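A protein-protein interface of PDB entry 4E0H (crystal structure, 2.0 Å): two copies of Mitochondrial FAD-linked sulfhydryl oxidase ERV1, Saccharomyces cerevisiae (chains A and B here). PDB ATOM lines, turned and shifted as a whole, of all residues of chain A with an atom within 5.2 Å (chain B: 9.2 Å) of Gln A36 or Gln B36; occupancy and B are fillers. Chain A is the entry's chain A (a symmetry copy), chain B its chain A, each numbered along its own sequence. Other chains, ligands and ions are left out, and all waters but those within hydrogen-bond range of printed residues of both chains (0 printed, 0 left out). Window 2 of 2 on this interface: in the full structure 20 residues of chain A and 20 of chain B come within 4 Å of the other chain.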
ATOM      1  N   GLY A  32      -8.906  16.263   2.724  1.00  0.00           N
ATOM      2  CA  GLY A  32      -9.264  16.971   3.961  1.00  0.00           C
ATOM      3  C   GLY A  32     -10.715  16.750   4.413  1.00  0.00           C
ATOM      4  O   GLY A  32     -10.997  16.665   5.609  1.00  0.00           O
ATOM      5  N   GLU A  33     -11.641  16.678   3.463  1.00  0.00           N
ATOM      6  CA  GLU A  33     -13.045  16.491   3.809  1.00  0.00           C
ATOM      7  C   GLU A  33     -13.291  15.068   4.236  1.00  0.00           C
ATOM      8  O   GLU A  33     -14.158  14.811   5.031  1.00  0.00           O
ATOM      9  CB  GLU A  33     -13.927  16.773   2.626  1.00  0.00           C
ATOM     10  CG  GLU A  33     -13.964  18.243   2.259  1.00  0.00           C
ATOM     11  CD  GLU A  33     -15.156  18.581   1.415  1.00  0.00           C
ATOM     12  OE1 GLU A  33     -15.841  17.638   0.943  1.00  0.00           O
ATOM     13  OE2 GLU A  33     -15.413  19.793   1.231  1.00  0.00           O
ATOM     14  N   MET A  34     -12.554  14.134   3.674  1.00  0.00           N
ATOM     15  CA  MET A  34     -12.718  12.741   4.106  1.00  0.00           C
ATOM     16  C   MET A  34     -12.271  12.574   5.591  1.00  0.00           C
ATOM     17  O   MET A  34     -12.973  11.986   6.424  1.00  0.00           O
ATOM     18  CB  MET A  34     -12.001  11.793   3.133  1.00  0.00           C
ATOM     19  CG  MET A  34     -12.125  10.312   3.544  1.00  0.00           C
ATOM     20  SD  MET A  34     -13.873   9.867   3.491  1.00  0.00           S
ATOM     21  CE  MET A  34     -14.150  10.052   1.739  1.00  0.00           C
ATOM     22  N   LYS A  35     -11.141  13.161   5.936  1.00  0.00           N
ATOM     23  CA  LYS A  35     -10.655  13.152   7.334  1.00  0.00           C
ATOM     24  C   LYS A  35     -11.672  13.779   8.293  1.00  0.00           C
ATOM     25  O   LYS A  35     -11.982  13.225   9.335  1.00  0.00           O
ATOM     26  CB  LYS A  35      -9.286  13.858   7.455  1.00  0.00           C
ATOM     27  CG  LYS A  35      -8.066  12.948   7.085  1.00  0.00           C
ATOM     28  CD  LYS A  35      -6.661  13.600   7.332  1.00  0.00           C
ATOM     29  CE  LYS A  35      -6.366  14.809   6.392  1.00  0.00           C
ATOM     30  NZ  LYS A  35      -4.935  15.271   6.476  1.00  0.00           N
ATOM     31  N   GLN A  36     -12.208  14.934   7.919  1.00  0.00           N
ATOM     32  CA  GLN A  36     -13.163  15.621   8.720  1.00  0.00           C
ATOM     33  C   GLN A  36     -14.453  14.838   8.769  1.00  0.00           C
ATOM     34  O   GLN A  36     -15.075  14.769   9.805  1.00  0.00           O
ATOM     35  CB  GLN A  36     -13.392  16.992   8.127  1.00  0.00           C
ATOM     36  CG  GLN A  36     -13.992  18.013   9.066  1.00  0.00           C
ATOM     37  CD  GLN A  36     -13.812  19.448   8.535  1.00  0.00           C
ATOM     38  OE1 GLN A  36     -14.058  19.747   7.343  1.00  0.00           O
ATOM     39  NE2 GLN A  36     -13.366  20.341   9.421  1.00  0.00           N
ATOM     40  N   PHE A  37     -14.869  14.247   7.648  1.00  0.00           N
ATOM     41  CA  PHE A  37     -16.082  13.479   7.648  1.00  0.00           C
ATOM     42  C   PHE A  37     -15.993  12.405   8.711  1.00  0.00           C
ATOM     43  O   PHE A  37     -16.895  12.190   9.539  1.00  0.00           O
ATOM     44  CB  PHE A  37     -16.246  12.794   6.312  1.00  0.00           C
ATOM     45  CG  PHE A  37     -17.520  11.983   6.216  1.00  0.00           C
ATOM     46  CD1 PHE A  37     -18.756  12.626   6.182  1.00  0.00           C
ATOM     47  CD2 PHE A  37     -17.471  10.588   6.152  1.00  0.00           C
ATOM     48  CE1 PHE A  37     -19.940  11.885   6.087  1.00  0.00           C
ATOM     49  CE2 PHE A  37     -18.651   9.835   6.035  1.00  0.00           C
ATOM     50  CZ  PHE A  37     -19.871  10.485   6.015  1.00  0.00           C
ATOM     51  N   LEU A  38     -14.874  11.699   8.663  1.00  0.00           N
ATOM     52  CA  LEU A  38     -14.684  10.557   9.545  1.00  0.00           C
ATOM     53  C   LEU A  38     -14.598  10.978  11.038  1.00  0.00           C
ATOM     54  O   LEU A  38     -15.177  10.345  11.914  1.00  0.00           O
ATOM     55  CB  LEU A  38     -13.478   9.748   9.069  1.00  0.00           C
ATOM     56  CG  LEU A  38     -13.627   8.880   7.822  1.00  0.00           C
ATOM     57  CD1 LEU A  38     -12.310   8.230   7.500  1.00  0.00           C
ATOM     58  CD2 LEU A  38     -14.669   7.797   7.984  1.00  0.00           C
ATOM     59  N   ASN A  39     -13.907  12.066  11.323  1.00  0.00           N
ATOM     60  CA  ASN A  39     -13.847  12.582  12.675  1.00  0.00           C
ATOM     61  C   ASN A  39     -15.225  12.931  13.176  1.00  0.00           C
ATOM     62  O   ASN A  39     -15.582  12.551  14.294  1.00  0.00           O
ATOM     63  CB  ASN A  39     -13.006  13.862  12.732  1.00  0.00           C
ATOM     64  CG  ASN A  39     -11.540  13.593  12.873  1.00  0.00           C
ATOM     65  OD1 ASN A  39     -11.107  12.476  13.174  1.00  0.00           O
ATOM     66  ND2 ASN A  39     -10.750  14.637  12.672  1.00  0.00           N
ATOM     67  N   ILE A  40     -15.995  13.664  12.365  1.00  0.00           N
ATOM     68  CA  ILE A  40     -17.326  14.082  12.802  1.00  0.00           C
ATOM     69  C   ILE A  40     -18.220  12.873  12.972  1.00  0.00           C
ATOM     70  O   ILE A  40     -18.964  12.778  13.958  1.00  0.00           O
ATOM     71  CB  ILE A  40     -17.959  15.062  11.846  1.00  0.00           C
ATOM     72  CG1 ILE A  40     -17.237  16.390  11.920  1.00  0.00           C
ATOM     73  CG2 ILE A  40     -19.402  15.317  12.251  1.00  0.00           C
ATOM     74  CD1 ILE A  40     -17.498  17.259  10.713  1.00  0.00           C
ATOM     75  N   PHE A  41     -18.130  11.933  12.031  1.00  0.00           N
ATOM     76  CA  PHE A  41     -18.925  10.696  12.127  1.00  0.00           C
ATOM     77  C   PHE A  41     -18.722  10.051  13.500  1.00  0.00           C
ATOM     78  O   PHE A  41     -19.677   9.638  14.173  1.00  0.00           O
ATOM     79  CB  PHE A  41     -18.502   9.725  11.018  1.00  0.00           C
ATOM     80  CG  PHE A  41     -19.257   8.416  11.052  1.00  0.00           C
ATOM     81  CD1 PHE A  41     -20.451   8.268  10.376  1.00  0.00           C
ATOM     82  CD2 PHE A  41     -18.758   7.336  11.756  1.00  0.00           C
ATOM     83  CE1 PHE A  41     -21.151   7.040  10.440  1.00  0.00           C
ATOM     84  CE2 PHE A  41     -19.462   6.115  11.817  1.00  0.00           C
ATOM     85  CZ  PHE A  41     -20.643   5.984  11.168  1.00  0.00           C
ATOM     86  N   GLN B  29     -20.662  23.999  19.357  1.00  0.00           N
ATOM     87  CA  GLN B  29     -19.843  23.023  18.640  1.00  0.00           C
ATOM     88  C   GLN B  29     -20.662  21.962  17.917  1.00  0.00           C
ATOM     89  O   GLN B  29     -20.327  21.583  16.814  1.00  0.00           O
ATOM     90  CB  GLN B  29     -18.873  22.324  19.601  1.00  0.00           C
ATOM     91  CG  GLN B  29     -18.111  21.142  18.976  1.00  0.00           C
ATOM     92  CD  GLN B  29     -16.992  21.604  18.051  1.00  0.00           C
ATOM     93  OE1 GLN B  29     -17.239  22.243  16.999  1.00  0.00           O
ATOM     94  NE2 GLN B  29     -15.742  21.295  18.444  1.00  0.00           N
ATOM     95  N   GLN B  30     -21.698  21.462  18.585  1.00  0.00           N
ATOM     96  CA  GLN B  30     -22.549  20.435  18.034  1.00  0.00           C
ATOM     97  C   GLN B  30     -23.250  21.002  16.808  1.00  0.00           C
ATOM     98  O   GLN B  30     -23.355  20.329  15.796  1.00  0.00           O
ATOM     99  CB  GLN B  30     -23.557  19.930  19.078  1.00  0.00           C
ATOM    100  CG  GLN B  30     -22.937  19.069  20.223  1.00  0.00           C
ATOM    101  CD  GLN B  30     -23.885  18.759  21.394  1.00  0.00           C
ATOM    102  OE1 GLN B  30     -24.552  19.620  21.929  1.00  0.00           O
ATOM    103  NE2 GLN B  30     -23.908  17.495  21.800  1.00  0.00           N
ATOM    104  N   LYS B  31     -23.708  22.246  16.877  1.00  0.00           N
ATOM    105  CA  LYS B  31     -24.325  22.878  15.725  1.00  0.00           C
ATOM    106  C   LYS B  31     -23.373  22.964  14.539  1.00  0.00           C
ATOM    107  O   LYS B  31     -23.757  22.679  13.429  1.00  0.00           O
ATOM    108  CB  LYS B  31     -24.819  24.306  16.057  1.00  0.00           C
ATOM    109  CG  LYS B  31     -25.922  24.367  17.060  1.00  0.00           C
ATOM    110  CD  LYS B  31     -26.311  25.786  17.320  1.00  0.00           C
ATOM    111  CE  LYS B  31     -27.020  25.842  18.631  1.00  0.00           C
ATOM    112  NZ  LYS B  31     -27.394  27.231  18.939  1.00  0.00           N
ATOM    113  N   GLY B  32     -22.133  23.370  14.775  1.00  0.00           N
ATOM    114  CA  GLY B  32     -21.179  23.545  13.671  1.00  0.00           C
ATOM    115  C   GLY B  32     -20.761  22.235  12.989  1.00  0.00           C
ATOM    116  O   GLY B  32     -20.566  22.190  11.774  1.00  0.00           O
ATOM    117  N   GLU B  33     -20.600  21.171  13.768  1.00  0.00           N
ATOM    118  CA  GLU B  33     -20.184  19.893  13.202  1.00  0.00           C
ATOM    119  C   GLU B  33     -21.330  19.251  12.465  1.00  0.00           C
ATOM    120  O   GLU B  33     -21.121  18.530  11.523  1.00  0.00           O
ATOM    121  CB  GLU B  33     -19.749  18.948  14.285  1.00  0.00           C
ATOM    122  CG  GLU B  33     -18.444  19.359  14.935  1.00  0.00           C
ATOM    123  CD  GLU B  33     -17.792  18.219  15.659  1.00  0.00           C
ATOM    124  OE1 GLU B  33     -18.454  17.164  15.831  1.00  0.00           O
ATOM    125  OE2 GLU B  33     -16.612  18.377  16.049  1.00  0.00           O
ATOM    126  N   MET B  34     -22.543  19.479  12.921  1.00  0.00           N
ATOM    127  CA  MET B  34     -23.692  18.924  12.196  1.00  0.00           C
ATOM    128  C   MET B  34     -23.813  19.574  10.784  1.00  0.00           C
ATOM    129  O   MET B  34     -23.966  18.895   9.761  1.00  0.00           O
ATOM    130  CB  MET B  34     -24.966  19.045  13.045  1.00  0.00           C
ATOM    131  CG  MET B  34     -26.214  18.491  12.329  1.00  0.00           C
ATOM    132  SD  MET B  34     -25.955  16.727  12.050  1.00  0.00           S
ATOM    133  CE  MET B  34     -25.920  16.183  13.748  1.00  0.00           C
ATOM    134  N   LYS B  35     -23.664  20.884  10.724  1.00  0.00           N
ATOM    135  CA  LYS B  35     -23.667  21.609   9.433  1.00  0.00           C
ATOM    136  C   LYS B  35     -22.573  21.098   8.491  1.00  0.00           C
ATOM    137  O   LYS B  35     -22.817  20.831   7.326  1.00  0.00           O
ATOM    138  CB  LYS B  35     -23.533  23.133   9.647  1.00  0.00           C
ATOM    139  CG  LYS B  35     -24.884  23.849   9.988  1.00  0.00           C
ATOM    140  CD  LYS B  35     -24.795  25.413  10.074  1.00  0.00           C
ATOM    141  CE  LYS B  35     -23.934  25.919  11.271  1.00  0.00           C
ATOM    142  NZ  LYS B  35     -24.051  27.406  11.480  1.00  0.00           N
ATOM    143  N   GLN B  36     -21.363  20.941   9.016  1.00  0.00           N
ATOM    144  CA  GLN B  36     -20.259  20.475   8.248  1.00  0.00           C
ATOM    145  C   GLN B  36     -20.471  19.030   7.865  1.00  0.00           C
ATOM    146  O   GLN B  36     -20.153  18.650   6.761  1.00  0.00           O
ATOM    147  CB  GLN B  36     -19.001  20.632   9.071  1.00  0.00           C
ATOM    148  CG  GLN B  36     -17.710  20.636   8.285  1.00  0.00           C
ATOM    149  CD  GLN B  36     -16.541  21.201   9.116  1.00  0.00           C
ATOM    150  OE1 GLN B  36     -16.337  20.840  10.300  1.00  0.00           O
ATOM    151  NE2 GLN B  36     -15.777  22.105   8.501  1.00  0.00           N
ATOM    152  N   PHE B  37     -21.004  18.214   8.774  1.00  0.00           N
ATOM    153  CA  PHE B  37     -21.239  16.835   8.451  1.00  0.00           C
ATOM    154  C   PHE B  37     -22.108  16.752   7.215  1.00  0.00           C
ATOM    155  O   PHE B  37     -21.844  16.021   6.245  1.00  0.00           O
ATOM    156  CB  PHE B  37     -21.984  16.170   9.585  1.00  0.00           C
ATOM    157  CG  PHE B  37     -22.247  14.701   9.339  1.00  0.00           C
ATOM    158  CD1 PHE B  37     -21.189  13.793   9.332  1.00  0.00           C
ATOM    159  CD2 PHE B  37     -23.549  14.239   9.123  1.00  0.00           C
ATOM    160  CE1 PHE B  37     -21.424  12.431   9.112  1.00  0.00           C
ATOM    161  CE2 PHE B  37     -23.798  12.872   8.922  1.00  0.00           C
ATOM    162  CZ  PHE B  37     -22.739  11.984   8.907  1.00  0.00           C
ATOM    163  N   LEU B  38     -23.189  17.513   7.271  1.00  0.00           N
ATOM    164  CA  LEU B  38     -24.184  17.462   6.210  1.00  0.00           C
ATOM    165  C   LEU B  38     -23.628  17.993   4.860  1.00  0.00           C
ATOM    166  O   LEU B  38     -23.863  17.419   3.803  1.00  0.00           O
ATOM    167  CB  LEU B  38     -25.452  18.179   6.673  1.00  0.00           C
ATOM    168  CG  LEU B  38     -26.357  17.482   7.685  1.00  0.00           C
ATOM    169  CD1 LEU B  38     -27.501  18.389   8.045  1.00  0.00           C
ATOM    170  CD2 LEU B  38     -26.923  16.181   7.164  1.00  0.00           C
ATOM    171  N   ASN B  39     -22.862  19.067   4.899  1.00  0.00           N
ATOM    172  CA  ASN B  39     -22.228  19.579   3.702  1.00  0.00           C
ATOM    173  C   ASN B  39     -21.311  18.547   3.098  1.00  0.00           C
ATOM    174  O   ASN B  39     -21.368  18.314   1.888  1.00  0.00           O
ATOM    175  CB  ASN B  39     -21.375  20.812   4.023  1.00  0.00           C
ATOM    176  CG  ASN B  39     -22.165  22.083   4.032  1.00  0.00           C
ATOM    177  OD1 ASN B  39     -23.311  22.144   3.573  1.00  0.00           O
ATOM    178  ND2 ASN B  39     -21.544  23.133   4.547  1.00  0.00           N
ATOM    179  N   ILE B  40     -20.456  17.939   3.928  1.00  0.00           N
ATOM    180  CA  ILE B  40     -19.504  16.960   3.408  1.00  0.00           C
ATOM    181  C   ILE B  40     -20.240  15.752   2.874  1.00  0.00           C
ATOM    182  O   ILE B  40     -19.906  15.238   1.797  1.00  0.00           O
ATOM    183  CB  ILE B  40     -18.497  16.535   4.446  1.00  0.00           C
ATOM    184  CG1 ILE B  40     -17.551  17.680   4.744  1.00  0.00           C
ATOM    185  CG2 ILE B  40     -17.653  15.391   3.908  1.00  0.00           C
ATOM    186  CD1 ILE B  40     -16.823  17.504   6.055  1.00  0.00           C
ATOM    187  N   PHE B  41     -21.261  15.309   3.607  1.00  0.00           N
ATOM    188  CA  PHE B  41     -22.072  14.165   3.154  1.00  0.00           C
ATOM    189  C   PHE B  41     -22.550  14.401   1.719  1.00  0.00           C
ATOM    190  O   PHE B  41     -22.468  13.520   0.853  1.00  0.00           O
ATOM    191  CB  PHE B  41     -23.273  13.981   4.090  1.00  0.00           C
ATOM    192  CG  PHE B  41     -24.173  12.836   3.687  1.00  0.00           C
ATOM    193  CD1 PHE B  41     -23.942  11.556   4.149  1.00  0.00           C
ATOM    194  CD2 PHE B  41     -25.254  13.052   2.853  1.00  0.00           C
ATOM    195  CE1 PHE B  41     -24.784  10.495   3.741  1.00  0.00           C
ATOM    196  CE2 PHE B  41     -26.090  11.990   2.450  1.00  0.00           C
ATOM    197  CZ  PHE B  41     -25.844  10.733   2.890  1.00  0.00           C
ATOM    198  N   SER B  42     -23.044  15.608   1.481  1.00  0.00           N
ATOM    199  CA  SER B  42     -23.567  15.965   0.171  1.00  0.00           C
ATOM    200  C   SER B  42     -22.470  15.999  -0.897  1.00  0.00           C
ATOM    201  O   SER B  42     -22.763  15.785  -2.070  1.00  0.00           O
ATOM    202  CB  SER B  42     -24.329  17.308   0.200  1.00  0.00           C
ATOM    203  OG  SER B  42     -23.424  18.403   0.249  1.00  0.00           O
ATOM    204  N   HIS B  43     -21.218  16.227  -0.514  1.00  0.00           N
ATOM    205  CA  HIS B  43     -20.158  16.178  -1.513  1.00  0.00           C
ATOM    206  C   HIS B  43     -19.767  14.753  -1.901  1.00  0.00           C
ATOM    207  O   HIS B  43     -19.536  14.467  -3.074  1.00  0.00           O
ATOM    208  CB  HIS B  43     -18.923  16.944  -1.069  1.00  0.00           C
ATOM    209  CG  HIS B  43     -19.164  18.393  -0.802  1.00  0.00           C
ATOM    210  ND1 HIS B  43     -18.348  19.146   0.021  1.00  0.00           N
ATOM    211  CD2 HIS B  43     -20.134  19.228  -1.236  1.00  0.00           C
ATOM    212  CE1 HIS B  43     -18.815  20.379   0.087  1.00  0.00           C
ATOM    213  NE2 HIS B  43     -19.893  20.456  -0.671  1.00  0.00           N
ATOM    214  N   ILE B  44     -19.723  13.869  -0.906  1.00  0.00           N
ATOM    215  CA  ILE B  44     -19.145  12.532  -1.060  1.00  0.00           C
ATOM    216  C   ILE B  44     -20.151  11.402  -1.214  1.00  0.00           C
ATOM    217  O   ILE B  44     -19.742  10.274  -1.400  1.00  0.00           O
ATOM    218  CB  ILE B  44     -18.201  12.210   0.121  1.00  0.00           C
ATOM    219  CG1 ILE B  44     -18.951  11.951   1.420  1.00  0.00           C
ATOM    220  CG2 ILE B  44     -17.167  13.303   0.320  1.00  0.00           C
ATOM    221  CD1 ILE B  44     -17.971  11.443   2.526  1.00  0.00           C
ATOM    222  N   ILE B  58     -29.249  21.562   0.237  1.00  0.00           N
ATOM    223  CA  ILE B  58     -28.613  22.155   1.402  1.00  0.00           C
ATOM    224  C   ILE B  58     -28.279  23.642   1.229  1.00  0.00           C
ATOM    225  O   ILE B  58     -28.426  24.428   2.176  1.00  0.00           O
ATOM    226  CB  ILE B  58     -27.364  21.371   1.805  1.00  0.00           C
ATOM    227  CG1 ILE B  58     -27.781  19.970   2.262  1.00  0.00           C
ATOM    228  CG2 ILE B  58     -26.586  22.134   2.876  1.00  0.00           C
ATOM    229  CD1 ILE B  58     -26.629  19.119   2.714  1.00  0.00           C
ATOM    230  N   PRO B  63     -29.544  23.473   6.385  1.00  0.00           N
ATOM    231  CA  PRO B  63     -29.894  22.653   7.557  1.00  0.00           C
ATOM    232  C   PRO B  63     -30.223  23.501   8.821  1.00  0.00           C
ATOM    233  O   PRO B  63     -29.482  24.416   9.184  1.00  0.00           O
ATOM    234  CB  PRO B  63     -28.657  21.760   7.743  1.00  0.00           C
ATOM    235  CG  PRO B  63     -28.030  21.671   6.350  1.00  0.00           C
ATOM    236  CD  PRO B  63     -28.314  23.013   5.708  1.00  0.00           C
ATOM    237  N   VAL B  65     -30.241  23.563  12.457  1.00  0.00           N
ATOM    238  CA  VAL B  65     -29.508  22.761  13.459  1.00  0.00           C
ATOM    239  C   VAL B  65     -29.659  23.311  14.873  1.00  0.00           C
ATOM    240  O   VAL B  65     -28.885  22.967  15.775  1.00  0.00           O
ATOM    241  CB  VAL B  65     -28.009  22.643  13.087  1.00  0.00           C
ATOM    242  CG1 VAL B  65     -27.836  21.992  11.742  1.00  0.00           C
ATOM    243  CG2 VAL B  65     -27.288  24.022  13.121  1.00  0.00           C
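Gln B36 touches its own counterpart, Gln A36.
Gln A36 touches Ile B40, and with the chains exchanged Ile A40 touches Gln B36.
Phe A37 touches its own counterpart, Phe B37.
Phe A37 touches Ile B40, and with the chains exchanged Ile A40 touches Phe B37.
10 positions are printed for both chains.
Of the 10 pairs that touch across the chains among the printed residues, 8 have their exchanged pair printed and touching as well.
Among the printed residues, merely in contact across the chains: Glu A33 with Ile B40 (3.7 Å), Gln A36 with Ile B40 (3.8 Å), Phe A37 with Phe B37 (3.4 Å), Phe A37 with Ile B40 (3.7 Å), Phe A37 with Ile B44 (3.8 Å), Ile A40 with Glu B33 (3.7 Å), Ile A40 with Gln B36 (3.8 Å) and Ile A40 with Phe B37 (3.7 Å).
Printed residues of chain B within 4 Å of Glu A33: Ile B40 (3.7 Å) and His B43 (3.1 Å).
Of chain B, only Gln B36 and Ile B40 come within 4 Å of Gln A36.
Printed residues of chain B within 4 Å of Phe A37: Phe B37, Ile B40 and Ile B44.
Of the printed residues of chain B, Ile A40 touches Glu B33 (3.7 Å), Gln B36 (3.8 Å) and Phe B37 (3.7 Å).
Gln B29 touches none of the printed residues of chain A.
Of the printed residues of chain A, Glu B33 touches Ile A40 (3.7 Å).
Gln B36 touches just these residues of chain A: Gln A36 and Ile A40.
Of the printed residues of chain A, Ile B44 touches Phe A37.
The nearest printed residue of chain A that does not touch Gln B36 is Phe A37 (6.2 Å).
The nearest printed residue of chain A that does not touch Glu B33 is Asn A39 (5.6 Å).
Printed residues of chain A that touch a printed residue of chain B: Glu A33, Gln A36, Phe A37 and Ile A40.
Hydrophobic or aromatic side chains of chain A that line the printed part of chain B: Phe A37 and Ile A40.
Hydrophobic or aromatic side chains of chain B within 4 Å of the printed part of chain A: Phe B37, Ile B40, His B43 and Ile B44.
Among the printed residues, no Asp or Glu carboxylate lies within 4 Å of a Lys or Arg side-chain nitrogen of the other chain.
NE2 of Gln A36 lies close to NE2 of Gln B36 (3.1 Å).
OE1 of Glu A33 sits at hydrogen-bond distance from ND1 of His B43 (3.1 Å).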
